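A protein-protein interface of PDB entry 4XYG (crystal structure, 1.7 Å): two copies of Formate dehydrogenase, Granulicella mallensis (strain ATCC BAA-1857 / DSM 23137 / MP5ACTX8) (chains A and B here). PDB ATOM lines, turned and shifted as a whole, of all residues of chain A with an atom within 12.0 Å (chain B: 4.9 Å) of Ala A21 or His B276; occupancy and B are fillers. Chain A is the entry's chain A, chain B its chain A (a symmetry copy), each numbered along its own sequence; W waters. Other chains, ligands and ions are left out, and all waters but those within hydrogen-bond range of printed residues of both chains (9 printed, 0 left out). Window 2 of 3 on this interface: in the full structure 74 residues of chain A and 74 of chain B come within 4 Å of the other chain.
O of Gly B277 lies within hydrogen-bond range of NH2 of Arg A22.
CB of Ala A21 touches NH1 of Arg B186, at 3.8 Å. Tyr B188 touches Ala A21. His B276 touches Ala A21 (CD2 to O, 3.4 Å). O of Ala A21 touches CA of Gly B277, 3.2 Å away. OH of Tyr B188 touches CG of Arg A22, at 3.3 Å. CG2 of Ile A25 touches CE1 of Tyr B188, at 3.7 Å. Leu A339 touches Tyr B188 (CD1 to CZ, 3.6 Å). Ser A340 touches Tyr B188 (OG to CA, 3.7 Å).
Water W7 lies within hydrogen-bond range of OH of Tyr B188 (2.5 Å), O of Gly A48 (2.8 Å) and O of Arg A22 (3.3 Å). Water W8 bridges the backbone carbonyl oxygen of Gly B301 (2.6 Å) and the backbone carbonyl oxygen of Ala A21 (2.7 Å). Water W1 lies within hydrogen-bond range of O of Leu A19 (2.6 Å) and NH1 of Arg B186 (2.6 Å). Water W2 lies within hydrogen-bond range of the guanidinium group (NH2) of Arg A22 (2.8 Å) and the side-chain hydroxyl (OG) of Ser B278 (2.9 Å). Water W3 bridges the backbone carbonyl oxygen (O) of His B276 and the backbone NH (N) of Asn A23. Water W5 bridges O of Tyr A20 (3.0 Å) and NE2 of His B276 (3.0 Å).
Printed residues of chain B that touch a printed residue of chain A: Arg B186, Tyr B188, His B276 and Gly B277. Along chain B the printed residues that touch a printed residue of chain A span positions 186 to 277. Hydrophobic or aromatic side chains of chain A within 4 Å of the printed part of chain B: Ala A21, Ile A25 and Leu A339. Among the printed residues, no Asp or Glu carboxylate lies within 4 Å of a Lys or Arg side-chain nitrogen of the other chain.
No position is printed for both chains.
N of Gly B277 is in hydrogen-bond range of O of Gln B302, 3.0 Å away. The backbone carbonyl oxygen (O) of Ala B304 sits at hydrogen-bond distance from the guanidinium group (NH2) of Arg B186. The backbone NH of Gly B277 is in hydrogen-bond range of the backbone carbonyl oxygen of Gly B301, 3.3 Å away.
Ala A21 touches just these residues of chain B: Arg B186, Tyr B188, His B276 and Gly B277. Of chain A, only Ala A21 (3.8 Å) comes within 4 Å of Arg B186. No residue of chain A comes within 4 Å of Arg B275. Gly B277 touches two residues of chain A. Ser B278 touches none of the printed residues of chain A. No residue of chain A comes within 4 Å of Ser B300. No residue of chain A comes within 4 Å of Gly B301. Gln B302 touches none of the printed residues of chain A. Printed residues of chain B within 4 Å of Arg A22: Tyr B188 and Gly B277. Of the printed residues of chain B, Ile A25 touches Tyr B188. Printed residues of chain B within 4 Å of Leu A339: Tyr B188. Printed residues of chain A within 4 Å of Tyr B188: Ala A21 (3.96 Å), Arg A22 (3.3 Å), Ile A25 (3.7 Å), Leu A339 (3.6 Å) and Ser A340 (3.7 Å).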
ATOM      1  N   PRO A  12      19.350  25.176 -38.205  1.00  0.00           N
ATOM      2  CA  PRO A  12      18.336  25.966 -37.499  1.00  0.00           C
ATOM      3  C   PRO A  12      18.535  27.458 -37.736  1.00  0.00           C
ATOM      4  O   PRO A  12      19.676  27.929 -37.825  1.00  0.00           O
ATOM      5  CB  PRO A  12      18.613  25.655 -36.027  1.00  0.00           C
ATOM      6  CG  PRO A  12      19.244  24.314 -36.031  1.00  0.00           C
ATOM      7  CD  PRO A  12      20.066  24.260 -37.293  1.00  0.00           C
ATOM      8  N   SER A  14      18.304  29.902 -35.735  1.00  0.00           N
ATOM      9  CA  SER A  14      19.101  30.522 -34.677  1.00  0.00           C
ATOM     10  C   SER A  14      20.559  30.036 -34.622  1.00  0.00           C
ATOM     11  O   SER A  14      21.329  30.466 -33.759  1.00  0.00           O
ATOM     12  CB  SER A  14      18.417  30.339 -33.317  1.00  0.00           C
ATOM     13  OG  SER A  14      17.990  29.001 -33.131  1.00  0.00           O
ATOM     14  N   GLY A  15      20.936  29.150 -35.543  1.00  0.00           N
ATOM     15  CA  GLY A  15      22.303  28.662 -35.620  1.00  0.00           C
ATOM     16  C   GLY A  15      22.499  27.257 -35.082  1.00  0.00           C
ATOM     17  O   GLY A  15      21.627  26.712 -34.404  1.00  0.00           O
ATOM     18  N   PRO A  17      25.059  24.593 -32.850  1.00  0.00           N
ATOM     19  CA  PRO A  17      23.968  23.686 -32.483  1.00  0.00           C
ATOM     20  C   PRO A  17      22.825  24.420 -31.802  1.00  0.00           C
ATOM     21  O   PRO A  17      23.025  25.512 -31.254  1.00  0.00           O
ATOM     22  CB  PRO A  17      24.637  22.737 -31.483  1.00  0.00           C
ATOM     23  CG  PRO A  17      25.671  23.581 -30.829  1.00  0.00           C
ATOM     24  CD  PRO A  17      26.182  24.505 -31.898  1.00  0.00           C
ATOM     25  N   PRO A  18      21.627  23.825 -31.829  1.00  0.00           N
ATOM     26  CA  PRO A  18      20.513  24.439 -31.108  1.00  0.00           C
ATOM     27  C   PRO A  18      20.692  24.222 -29.616  1.00  0.00           C
ATOM     28  O   PRO A  18      21.549  23.437 -29.205  1.00  0.00           O
ATOM     29  CB  PRO A  18      19.305  23.645 -31.611  1.00  0.00           C
ATOM     30  CG  PRO A  18      19.860  22.284 -31.909  1.00  0.00           C
ATOM     31  CD  PRO A  18      21.256  22.532 -32.443  1.00  0.00           C
ATOM     32  N   LEU A  19      19.893  24.900 -28.798  1.00  0.00           N
ATOM     33  CA  LEU A  19      19.917  24.647 -27.362  1.00  0.00           C
ATOM     34  C   LEU A  19      19.028  23.453 -27.033  1.00  0.00           C
ATOM     35  O   LEU A  19      17.805  23.553 -27.091  1.00  0.00           O
ATOM     36  CB  LEU A  19      19.440  25.870 -26.578  1.00  0.00           C
ATOM     37  CG  LEU A  19      19.267  25.627 -25.076  1.00  0.00           C
ATOM     38  CD1 LEU A  19      20.618  25.399 -24.408  1.00  0.00           C
ATOM     39  CD2 LEU A  19      18.503  26.762 -24.403  1.00  0.00           C
ATOM     40  N   TYR A  20      19.639  22.323 -26.699  1.00  0.00           N
ATOM     41  CA  TYR A  20      18.866  21.099 -26.489  1.00  0.00           C
ATOM     42  C   TYR A  20      18.062  21.178 -25.197  1.00  0.00           C
ATOM     43  O   TYR A  20      18.544  21.672 -24.174  1.00  0.00           O
ATOM     44  CB  TYR A  20      19.777  19.874 -26.487  1.00  0.00           C
ATOM     45  CG  TYR A  20      20.503  19.680 -27.801  1.00  0.00           C
ATOM     46  CD1 TYR A  20      19.811  19.295 -28.947  1.00  0.00           C
ATOM     47  CD2 TYR A  20      21.877  19.886 -27.895  1.00  0.00           C
ATOM     48  CE1 TYR A  20      20.470  19.121 -30.154  1.00  0.00           C
ATOM     49  CE2 TYR A  20      22.543  19.718 -29.094  1.00  0.00           C
ATOM     50  CZ  TYR A  20      21.837  19.335 -30.218  1.00  0.00           C
ATOM     51  OH  TYR A  20      22.500  19.166 -31.422  1.00  0.00           O
ATOM     52  N   ALA A  21      16.824  20.697 -25.270  1.00  0.00           N
ATOM     53  CA  ALA A  21      15.922  20.623 -24.125  1.00  0.00           C
ATOM     54  C   ALA A  21      16.379  19.611 -23.083  1.00  0.00           C
ATOM     55  O   ALA A  21      16.095  19.765 -21.891  1.00  0.00           O
ATOM     56  CB  ALA A  21      14.518  20.287 -24.607  1.00  0.00           C
ATOM     57  N   ARG A  22      17.056  18.558 -23.537  1.00  0.00           N
ATOM     58  CA  ARG A  22      17.539  17.503 -22.645  1.00  0.00           C
ATOM     59  C   ARG A  22      18.878  16.977 -23.145  1.00  0.00           C
ATOM     60  O   ARG A  22      19.243  17.207 -24.292  1.00  0.00           O
ATOM     61  CB  ARG A  22      16.524  16.355 -22.553  1.00  0.00           C
ATOM     62  CG  ARG A  22      16.182  15.733 -23.910  1.00  0.00           C
ATOM     63  CD  ARG A  22      15.350  14.444 -23.766  1.00  0.00           C
ATOM     64  NE  ARG A  22      14.192  14.658 -22.917  1.00  0.00           N
ATOM     65  CZ  ARG A  22      13.793  13.847 -21.941  1.00  0.00           C
ATOM     66  NH1 ARG A  22      14.441  12.713 -21.660  1.00  0.00           N
ATOM     67  NH2 ARG A  22      12.722  14.179 -21.246  1.00  0.00           N
ATOM     68  N   ASN A  23      19.616  16.266 -22.301  1.00  0.00           N
ATOM     69  CA  ASN A  23      20.932  15.807 -22.731  1.00  0.00           C
ATOM     70  C   ASN A  23      21.041  14.304 -22.947  1.00  0.00           C
ATOM     71  O   ASN A  23      22.132  13.794 -23.220  1.00  0.00           O
ATOM     72  CB  ASN A  23      22.023  16.297 -21.778  1.00  0.00           C
ATOM     73  CG  ASN A  23      21.787  15.867 -20.353  1.00  0.00           C
ATOM     74  OD1 ASN A  23      21.309  14.763 -20.091  1.00  0.00           O
ATOM     75  ND2 ASN A  23      22.114  16.751 -19.409  1.00  0.00           N
ATOM     76  N   ALA A  24      19.918  13.596 -22.819  1.00  0.00           N
ATOM     77  CA  ALA A  24      19.890  12.158 -23.101  1.00  0.00           C
ATOM     78  C   ALA A  24      18.514  11.746 -23.613  1.00  0.00           C
ATOM     79  O   ALA A  24      17.521  12.387 -23.294  1.00  0.00           O
ATOM     80  CB  ALA A  24      20.243  11.367 -21.864  1.00  0.00           C
ATOM     81  N   ILE A  25      18.464  10.682 -24.410  1.00  0.00           N
ATOM     82  CA  ILE A  25      17.188  10.120 -24.869  1.00  0.00           C
ATOM     83  C   ILE A  25      17.138   8.628 -24.533  1.00  0.00           C
ATOM     84  O   ILE A  25      18.177   8.019 -24.241  1.00  0.00           O
ATOM     85  CB  ILE A  25      16.980  10.335 -26.390  1.00  0.00           C
ATOM     86  CG1 ILE A  25      18.114   9.697 -27.188  1.00  0.00           C
ATOM     87  CG2 ILE A  25      16.881  11.818 -26.717  1.00  0.00           C
ATOM     88  CD1 ILE A  25      17.855   9.696 -28.695  1.00  0.00           C
ATOM     89  N   PRO A  26      15.930   8.026 -24.551  1.00  0.00           N
ATOM     90  CA  PRO A  26      15.837   6.588 -24.271  1.00  0.00           C
ATOM     91  C   PRO A  26      16.716   5.744 -25.191  1.00  0.00           C
ATOM     92  O   PRO A  26      16.893   6.088 -26.360  1.00  0.00           O
ATOM     93  CB  PRO A  26      14.361   6.286 -24.544  1.00  0.00           C
ATOM     94  CG  PRO A  26      13.657   7.558 -24.175  1.00  0.00           C
ATOM     95  CD  PRO A  26      14.593   8.645 -24.681  1.00  0.00           C
ATOM     96  N   VAL A  46      26.302  12.144 -29.470  1.00  0.00           N
ATOM     97  CA  VAL A  46      25.491  11.730 -28.336  1.00  0.00           C
ATOM     98  C   VAL A  46      24.060  11.655 -28.848  1.00  0.00           C
ATOM     99  O   VAL A  46      23.552  12.632 -29.395  1.00  0.00           O
ATOM    100  CB  VAL A  46      25.578  12.748 -27.186  1.00  0.00           C
ATOM    101  CG1 VAL A  46      24.684  12.327 -26.029  1.00  0.00           C
ATOM    102  CG2 VAL A  46      27.009  12.885 -26.703  1.00  0.00           C
ATOM    103  N   PRO A  47      23.422  10.479 -28.723  1.00  0.00           N
ATOM    104  CA  PRO A  47      22.039  10.368 -29.205  1.00  0.00           C
ATOM    105  C   PRO A  47      21.186  11.465 -28.578  1.00  0.00           C
ATOM    106  O   PRO A  47      21.238  11.684 -27.360  1.00  0.00           O
ATOM    107  CB  PRO A  47      21.608   8.989 -28.713  1.00  0.00           C
ATOM    108  CG  PRO A  47      22.920   8.202 -28.649  1.00  0.00           C
ATOM    109  CD  PRO A  47      23.917   9.219 -28.147  1.00  0.00           C
ATOM    110  N   GLY A  48      20.441  12.167 -29.420  1.00  0.00           N
ATOM    111  CA  GLY A  48      19.736  13.358 -28.998  1.00  0.00           C
ATOM    112  C   GLY A  48      20.213  14.571 -29.777  1.00  0.00           C
ATOM    113  O   GLY A  48      19.490  15.560 -29.906  1.00  0.00           O
ATOM    114  N   GLU A  49      21.428  14.500 -30.319  1.00  0.00           N
ATOM    115  CA  GLU A  49      21.937  15.620 -31.106  1.00  0.00           C
ATOM    116  C   GLU A  49      21.212  15.794 -32.442  1.00  0.00           C
ATOM    117  O   GLU A  49      20.688  14.830 -33.032  1.00  0.00           O
ATOM    118  CB  GLU A  49      23.447  15.478 -31.341  1.00  0.00           C
ATOM    119  CG  GLU A  49      24.324  15.787 -30.131  1.00  0.00           C
ATOM    120  CD  GLU A  49      25.808  15.796 -30.490  1.00  0.00           C
ATOM    121  OE1 GLU A  49      26.522  14.847 -30.104  1.00  0.00           O
ATOM    122  OE2 GLU A  49      26.253  16.749 -31.171  1.00  0.00           O
ATOM    123  N   LEU A  50      21.180  17.034 -32.923  1.00  0.00           N
ATOM    124  CA  LEU A  50      20.624  17.337 -34.229  1.00  0.00           C
ATOM    125  C   LEU A  50      21.625  16.914 -35.308  1.00  0.00           C
ATOM    126  O   LEU A  50      22.725  17.462 -35.394  1.00  0.00           O
ATOM    127  CB  LEU A  50      20.303  18.833 -34.343  1.00  0.00           C
ATOM    128  CG  LEU A  50      19.784  19.304 -35.705  1.00  0.00           C
ATOM    129  CD1 LEU A  50      18.564  18.513 -36.187  1.00  0.00           C
ATOM    130  CD2 LEU A  50      19.450  20.786 -35.684  1.00  0.00           C
ATOM    131  N   SER A 338      12.417  13.253 -35.958  1.00  0.00           N
ATOM    132  CA  SER A 338      12.558  13.544 -34.526  1.00  0.00           C
ATOM    133  C   SER A 338      14.014  13.272 -34.128  1.00  0.00           C
ATOM    134  O   SER A 338      14.700  12.486 -34.788  1.00  0.00           O
ATOM    135  CB  SER A 338      11.619  12.673 -33.686  1.00  0.00           C
ATOM    136  OG  SER A 338      12.035  11.314 -33.689  1.00  0.00           O
ATOM    137  N   LEU A 339      14.502  13.940 -33.085  1.00  0.00           N
ATOM    138  CA  LEU A 339      15.873  13.700 -32.633  1.00  0.00           C
ATOM    139  C   LEU A 339      16.093  12.218 -32.308  1.00  0.00           C
ATOM    140  O   LEU A 339      17.184  11.675 -32.521  1.00  0.00           O
ATOM    141  CB  LEU A 339      16.211  14.601 -31.437  1.00  0.00           C
ATOM    142  CG  LEU A 339      16.131  16.084 -31.809  1.00  0.00           C
ATOM    143  CD1 LEU A 339      16.166  16.983 -30.556  1.00  0.00           C
ATOM    144  CD2 LEU A 339      17.271  16.444 -32.763  1.00  0.00           C
ATOM    145  N   SER A 340      15.034  11.559 -31.831  1.00  0.00           N
ATOM    146  CA  SER A 340      15.106  10.153 -31.484  1.00  0.00           C
ATOM    147  C   SER A 340      15.303   9.298 -32.735  1.00  0.00           C
ATOM    148  O   SER A 340      16.143   8.393 -32.744  1.00  0.00           O
ATOM    149  CB  SER A 340      13.840   9.744 -30.725  1.00  0.00           C
ATOM    150  OG  SER A 340      13.592  10.685 -29.680  1.00  0.00           O
ATOM    151  N   ARG B 186      13.399  20.425 -31.073  1.00  0.00           N
ATOM    152  CA  ARG B 186      12.843  20.038 -29.779  1.00  0.00           C
ATOM    153  C   ARG B 186      11.869  18.873 -29.899  1.00  0.00           C
ATOM    154  O   ARG B 186      11.020  18.692 -29.025  1.00  0.00           O
ATOM    155  CB  ARG B 186      12.106  21.218 -29.120  1.00  0.00           C
ATOM    156  CG  ARG B 186      12.903  22.498 -28.983  1.00  0.00           C
ATOM    157  CD  ARG B 186      12.024  23.599 -28.384  1.00  0.00           C
ATOM    158  NE  ARG B 186      11.416  23.159 -27.131  1.00  0.00           N
ATOM    159  CZ  ARG B 186      12.040  23.195 -25.957  1.00  0.00           C
ATOM    160  NH1 ARG B 186      13.283  23.650 -25.892  1.00  0.00           N
ATOM    161  NH2 ARG B 186      11.429  22.776 -24.848  1.00  0.00           N
ATOM    162  N   TYR B 188      10.954  14.952 -29.937  1.00  0.00           N
ATOM    163  CA  TYR B 188      11.393  13.634 -29.471  1.00  0.00           C
ATOM    164  C   TYR B 188      10.257  12.639 -29.649  1.00  0.00           C
ATOM    165  O   TYR B 188       9.099  13.031 -29.750  1.00  0.00           O
ATOM    166  CB  TYR B 188      11.781  13.678 -27.984  1.00  0.00           C
ATOM    167  CG  TYR B 188      12.932  14.607 -27.686  1.00  0.00           C
ATOM    168  CD1 TYR B 188      14.241  14.174 -27.815  1.00  0.00           C
ATOM    169  CD2 TYR B 188      12.703  15.913 -27.280  1.00  0.00           C
ATOM    170  CE1 TYR B 188      15.295  15.015 -27.549  1.00  0.00           C
ATOM    171  CE2 TYR B 188      13.759  16.778 -27.022  1.00  0.00           C
ATOM    172  CZ  TYR B 188      15.051  16.314 -27.157  1.00  0.00           C
ATOM    173  OH  TYR B 188      16.120  17.155 -26.900  1.00  0.00           O
ATOM    174  N   MET B 274      13.109  16.319 -10.738  1.00  0.00           N
ATOM    175  CA  MET B 274      13.020  15.745 -12.078  1.00  0.00           C
ATOM    176  C   MET B 274      14.278  16.036 -12.877  1.00  0.00           C
ATOM    177  O   MET B 274      14.995  16.997 -12.598  1.00  0.00           O
ATOM    178  CB  MET B 274      11.805  16.303 -12.818  1.00  0.00           C
ATOM    179  CG  MET B 274      10.479  16.008 -12.142  1.00  0.00           C
ATOM    180  SD  MET B 274       9.089  16.420 -13.214  1.00  0.00           S
ATOM    181  CE  MET B 274       8.934  14.928 -14.219  1.00  0.00           C
ATOM    182  N   ARG B 275      14.549  15.202 -13.874  1.00  0.00           N
ATOM    183  CA  ARG B 275      15.654  15.458 -14.782  1.00  0.00           C
ATOM    184  C   ARG B 275      15.366  16.724 -15.582  1.00  0.00           C
ATOM    185  O   ARG B 275      14.226  16.982 -15.963  1.00  0.00           O
ATOM    186  CB  ARG B 275      15.846  14.265 -15.711  1.00  0.00           C
ATOM    187  CG  ARG B 275      17.231  14.141 -16.314  1.00  0.00           C
ATOM    188  CD  ARG B 275      17.472  12.702 -16.745  1.00  0.00           C
ATOM    189  NE  ARG B 275      17.231  11.770 -15.647  1.00  0.00           N
ATOM    190  CZ  ARG B 275      18.158  11.401 -14.768  1.00  0.00           C
ATOM    191  NH1 ARG B 275      19.392  11.878 -14.869  1.00  0.00           N
ATOM    192  NH2 ARG B 275      17.857  10.553 -13.795  1.00  0.00           N
ATOM    193  N   HIS B 276      16.395  17.532 -15.811  1.00  0.00           N
ATOM    194  CA  HIS B 276      16.257  18.733 -16.625  1.00  0.00           C
ATOM    195  C   HIS B 276      15.686  18.389 -18.005  1.00  0.00           C
ATOM    196  O   HIS B 276      16.227  17.533 -18.706  1.00  0.00           O
ATOM    197  CB  HIS B 276      17.628  19.386 -16.778  1.00  0.00           C
ATOM    198  CG  HIS B 276      17.641  20.573 -17.686  1.00  0.00           C
ATOM    199  ND1 HIS B 276      17.551  21.867 -17.220  1.00  0.00           N
ATOM    200  CD2 HIS B 276      17.750  20.663 -19.033  1.00  0.00           C
ATOM    201  CE1 HIS B 276      17.599  22.703 -18.241  1.00  0.00           C
ATOM    202  NE2 HIS B 276      17.716  21.999 -19.354  1.00  0.00           N
ATOM    203  N   GLY B 277      14.589  19.038 -18.385  1.00  0.00           N
ATOM    204  CA  GLY B 277      13.970  18.770 -19.676  1.00  0.00           C
ATOM    205  C   GLY B 277      12.821  17.775 -19.599  1.00  0.00           C
ATOM    206  O   GLY B 277      12.468  17.144 -20.603  1.00  0.00           O
ATOM    207  N   SER B 278      12.217  17.649 -18.422  1.00  0.00           N
ATOM    208  CA  SER B 278      11.059  16.767 -18.249  1.00  0.00           C
ATOM    209  C   SER B 278       9.756  17.458 -18.652  1.00  0.00           C
ATOM    210  O   SER B 278       9.727  18.668 -18.921  1.00  0.00           O
ATOM    211  CB  SER B 278      10.966  16.279 -16.801  1.00  0.00           C
ATOM    212  OG  SER B 278      12.063  15.455 -16.456  1.00  0.00           O
ATOM    213  N   SER B 300      13.606  28.296 -17.132  1.00  0.00           N
ATOM    214  CA  SER B 300      14.949  27.777 -16.880  1.00  0.00           C
ATOM    215  C   SER B 300      15.248  26.536 -17.716  1.00  0.00           C
ATOM    216  O   SER B 300      16.410  26.165 -17.908  1.00  0.00           O
ATOM    217  CB  SER B 300      15.116  27.429 -15.407  1.00  0.00           C
ATOM    218  OG  SER B 300      14.435  26.228 -15.081  1.00  0.00           O
ATOM    219  N   GLY B 301      14.193  25.884 -18.198  1.00  0.00           N
ATOM    220  CA  GLY B 301      14.353  24.654 -18.948  1.00  0.00           C
ATOM    221  C   GLY B 301      14.245  23.412 -18.086  1.00  0.00           C
ATOM    222  O   GLY B 301      14.307  22.295 -18.604  1.00  0.00           O
ATOM    223  N   GLN B 302      14.089  23.589 -16.774  1.00  0.00           N
ATOM    224  CA  GLN B 302      13.888  22.452 -15.887  1.00  0.00           C
ATOM    225  C   GLN B 302      12.724  21.596 -16.403  1.00  0.00           C
ATOM    226  O   GLN B 302      12.808  20.369 -16.422  1.00  0.00           O
ATOM    227  CB  GLN B 302      13.647  22.908 -14.444  1.00  0.00           C
ATOM    228  CG  GLN B 302      13.402  21.763 -13.456  1.00  0.00           C
ATOM    229  CD  GLN B 302      14.567  20.790 -13.359  1.00  0.00           C
ATOM    230  OE1 GLN B 302      15.725  21.153 -13.577  1.00  0.00           O
ATOM    231  NE2 GLN B 302      14.259  19.538 -13.055  1.00  0.00           N
ATOM    232  N   ALA B 304      10.783  20.933 -19.972  1.00  0.00           N
ATOM    233  CA  ALA B 304      10.826  21.163 -21.410  1.00  0.00           C
ATOM    234  C   ALA B 304       9.448  21.543 -21.933  1.00  0.00           C
ATOM    235  O   ALA B 304       9.326  22.068 -23.036  1.00  0.00           O
ATOM    236  CB  ALA B 304      11.348  19.916 -22.139  1.00  0.00           C
HETATM  237  O   HOH W   1      15.690  24.626 -26.035  1.00  0.00           O
HETATM  238  O   HOH W   2      13.379  13.943 -18.547  1.00  0.00           O
HETATM  239  O   HOH W   3      18.811  16.823 -19.477  1.00  0.00           O
HETATM  240  O   HOH W   4      15.857  19.802 -27.746  1.00  0.00           O
HETATM  241  O   HOH W   5      17.786  23.507 -21.951  1.00  0.00           O
HETATM  242  O   HOH W   6      13.077  17.193 -23.276  1.00  0.00           O
HETATM  243  O   HOH W   7      18.434  16.235 -27.354  1.00  0.00           O
HETATM  244  O   HOH W   8      14.402  21.759 -21.136  1.00  0.00           O
HETATM  245  O   HOH W   9      15.659  14.954 -19.437  1.00  0.00           O
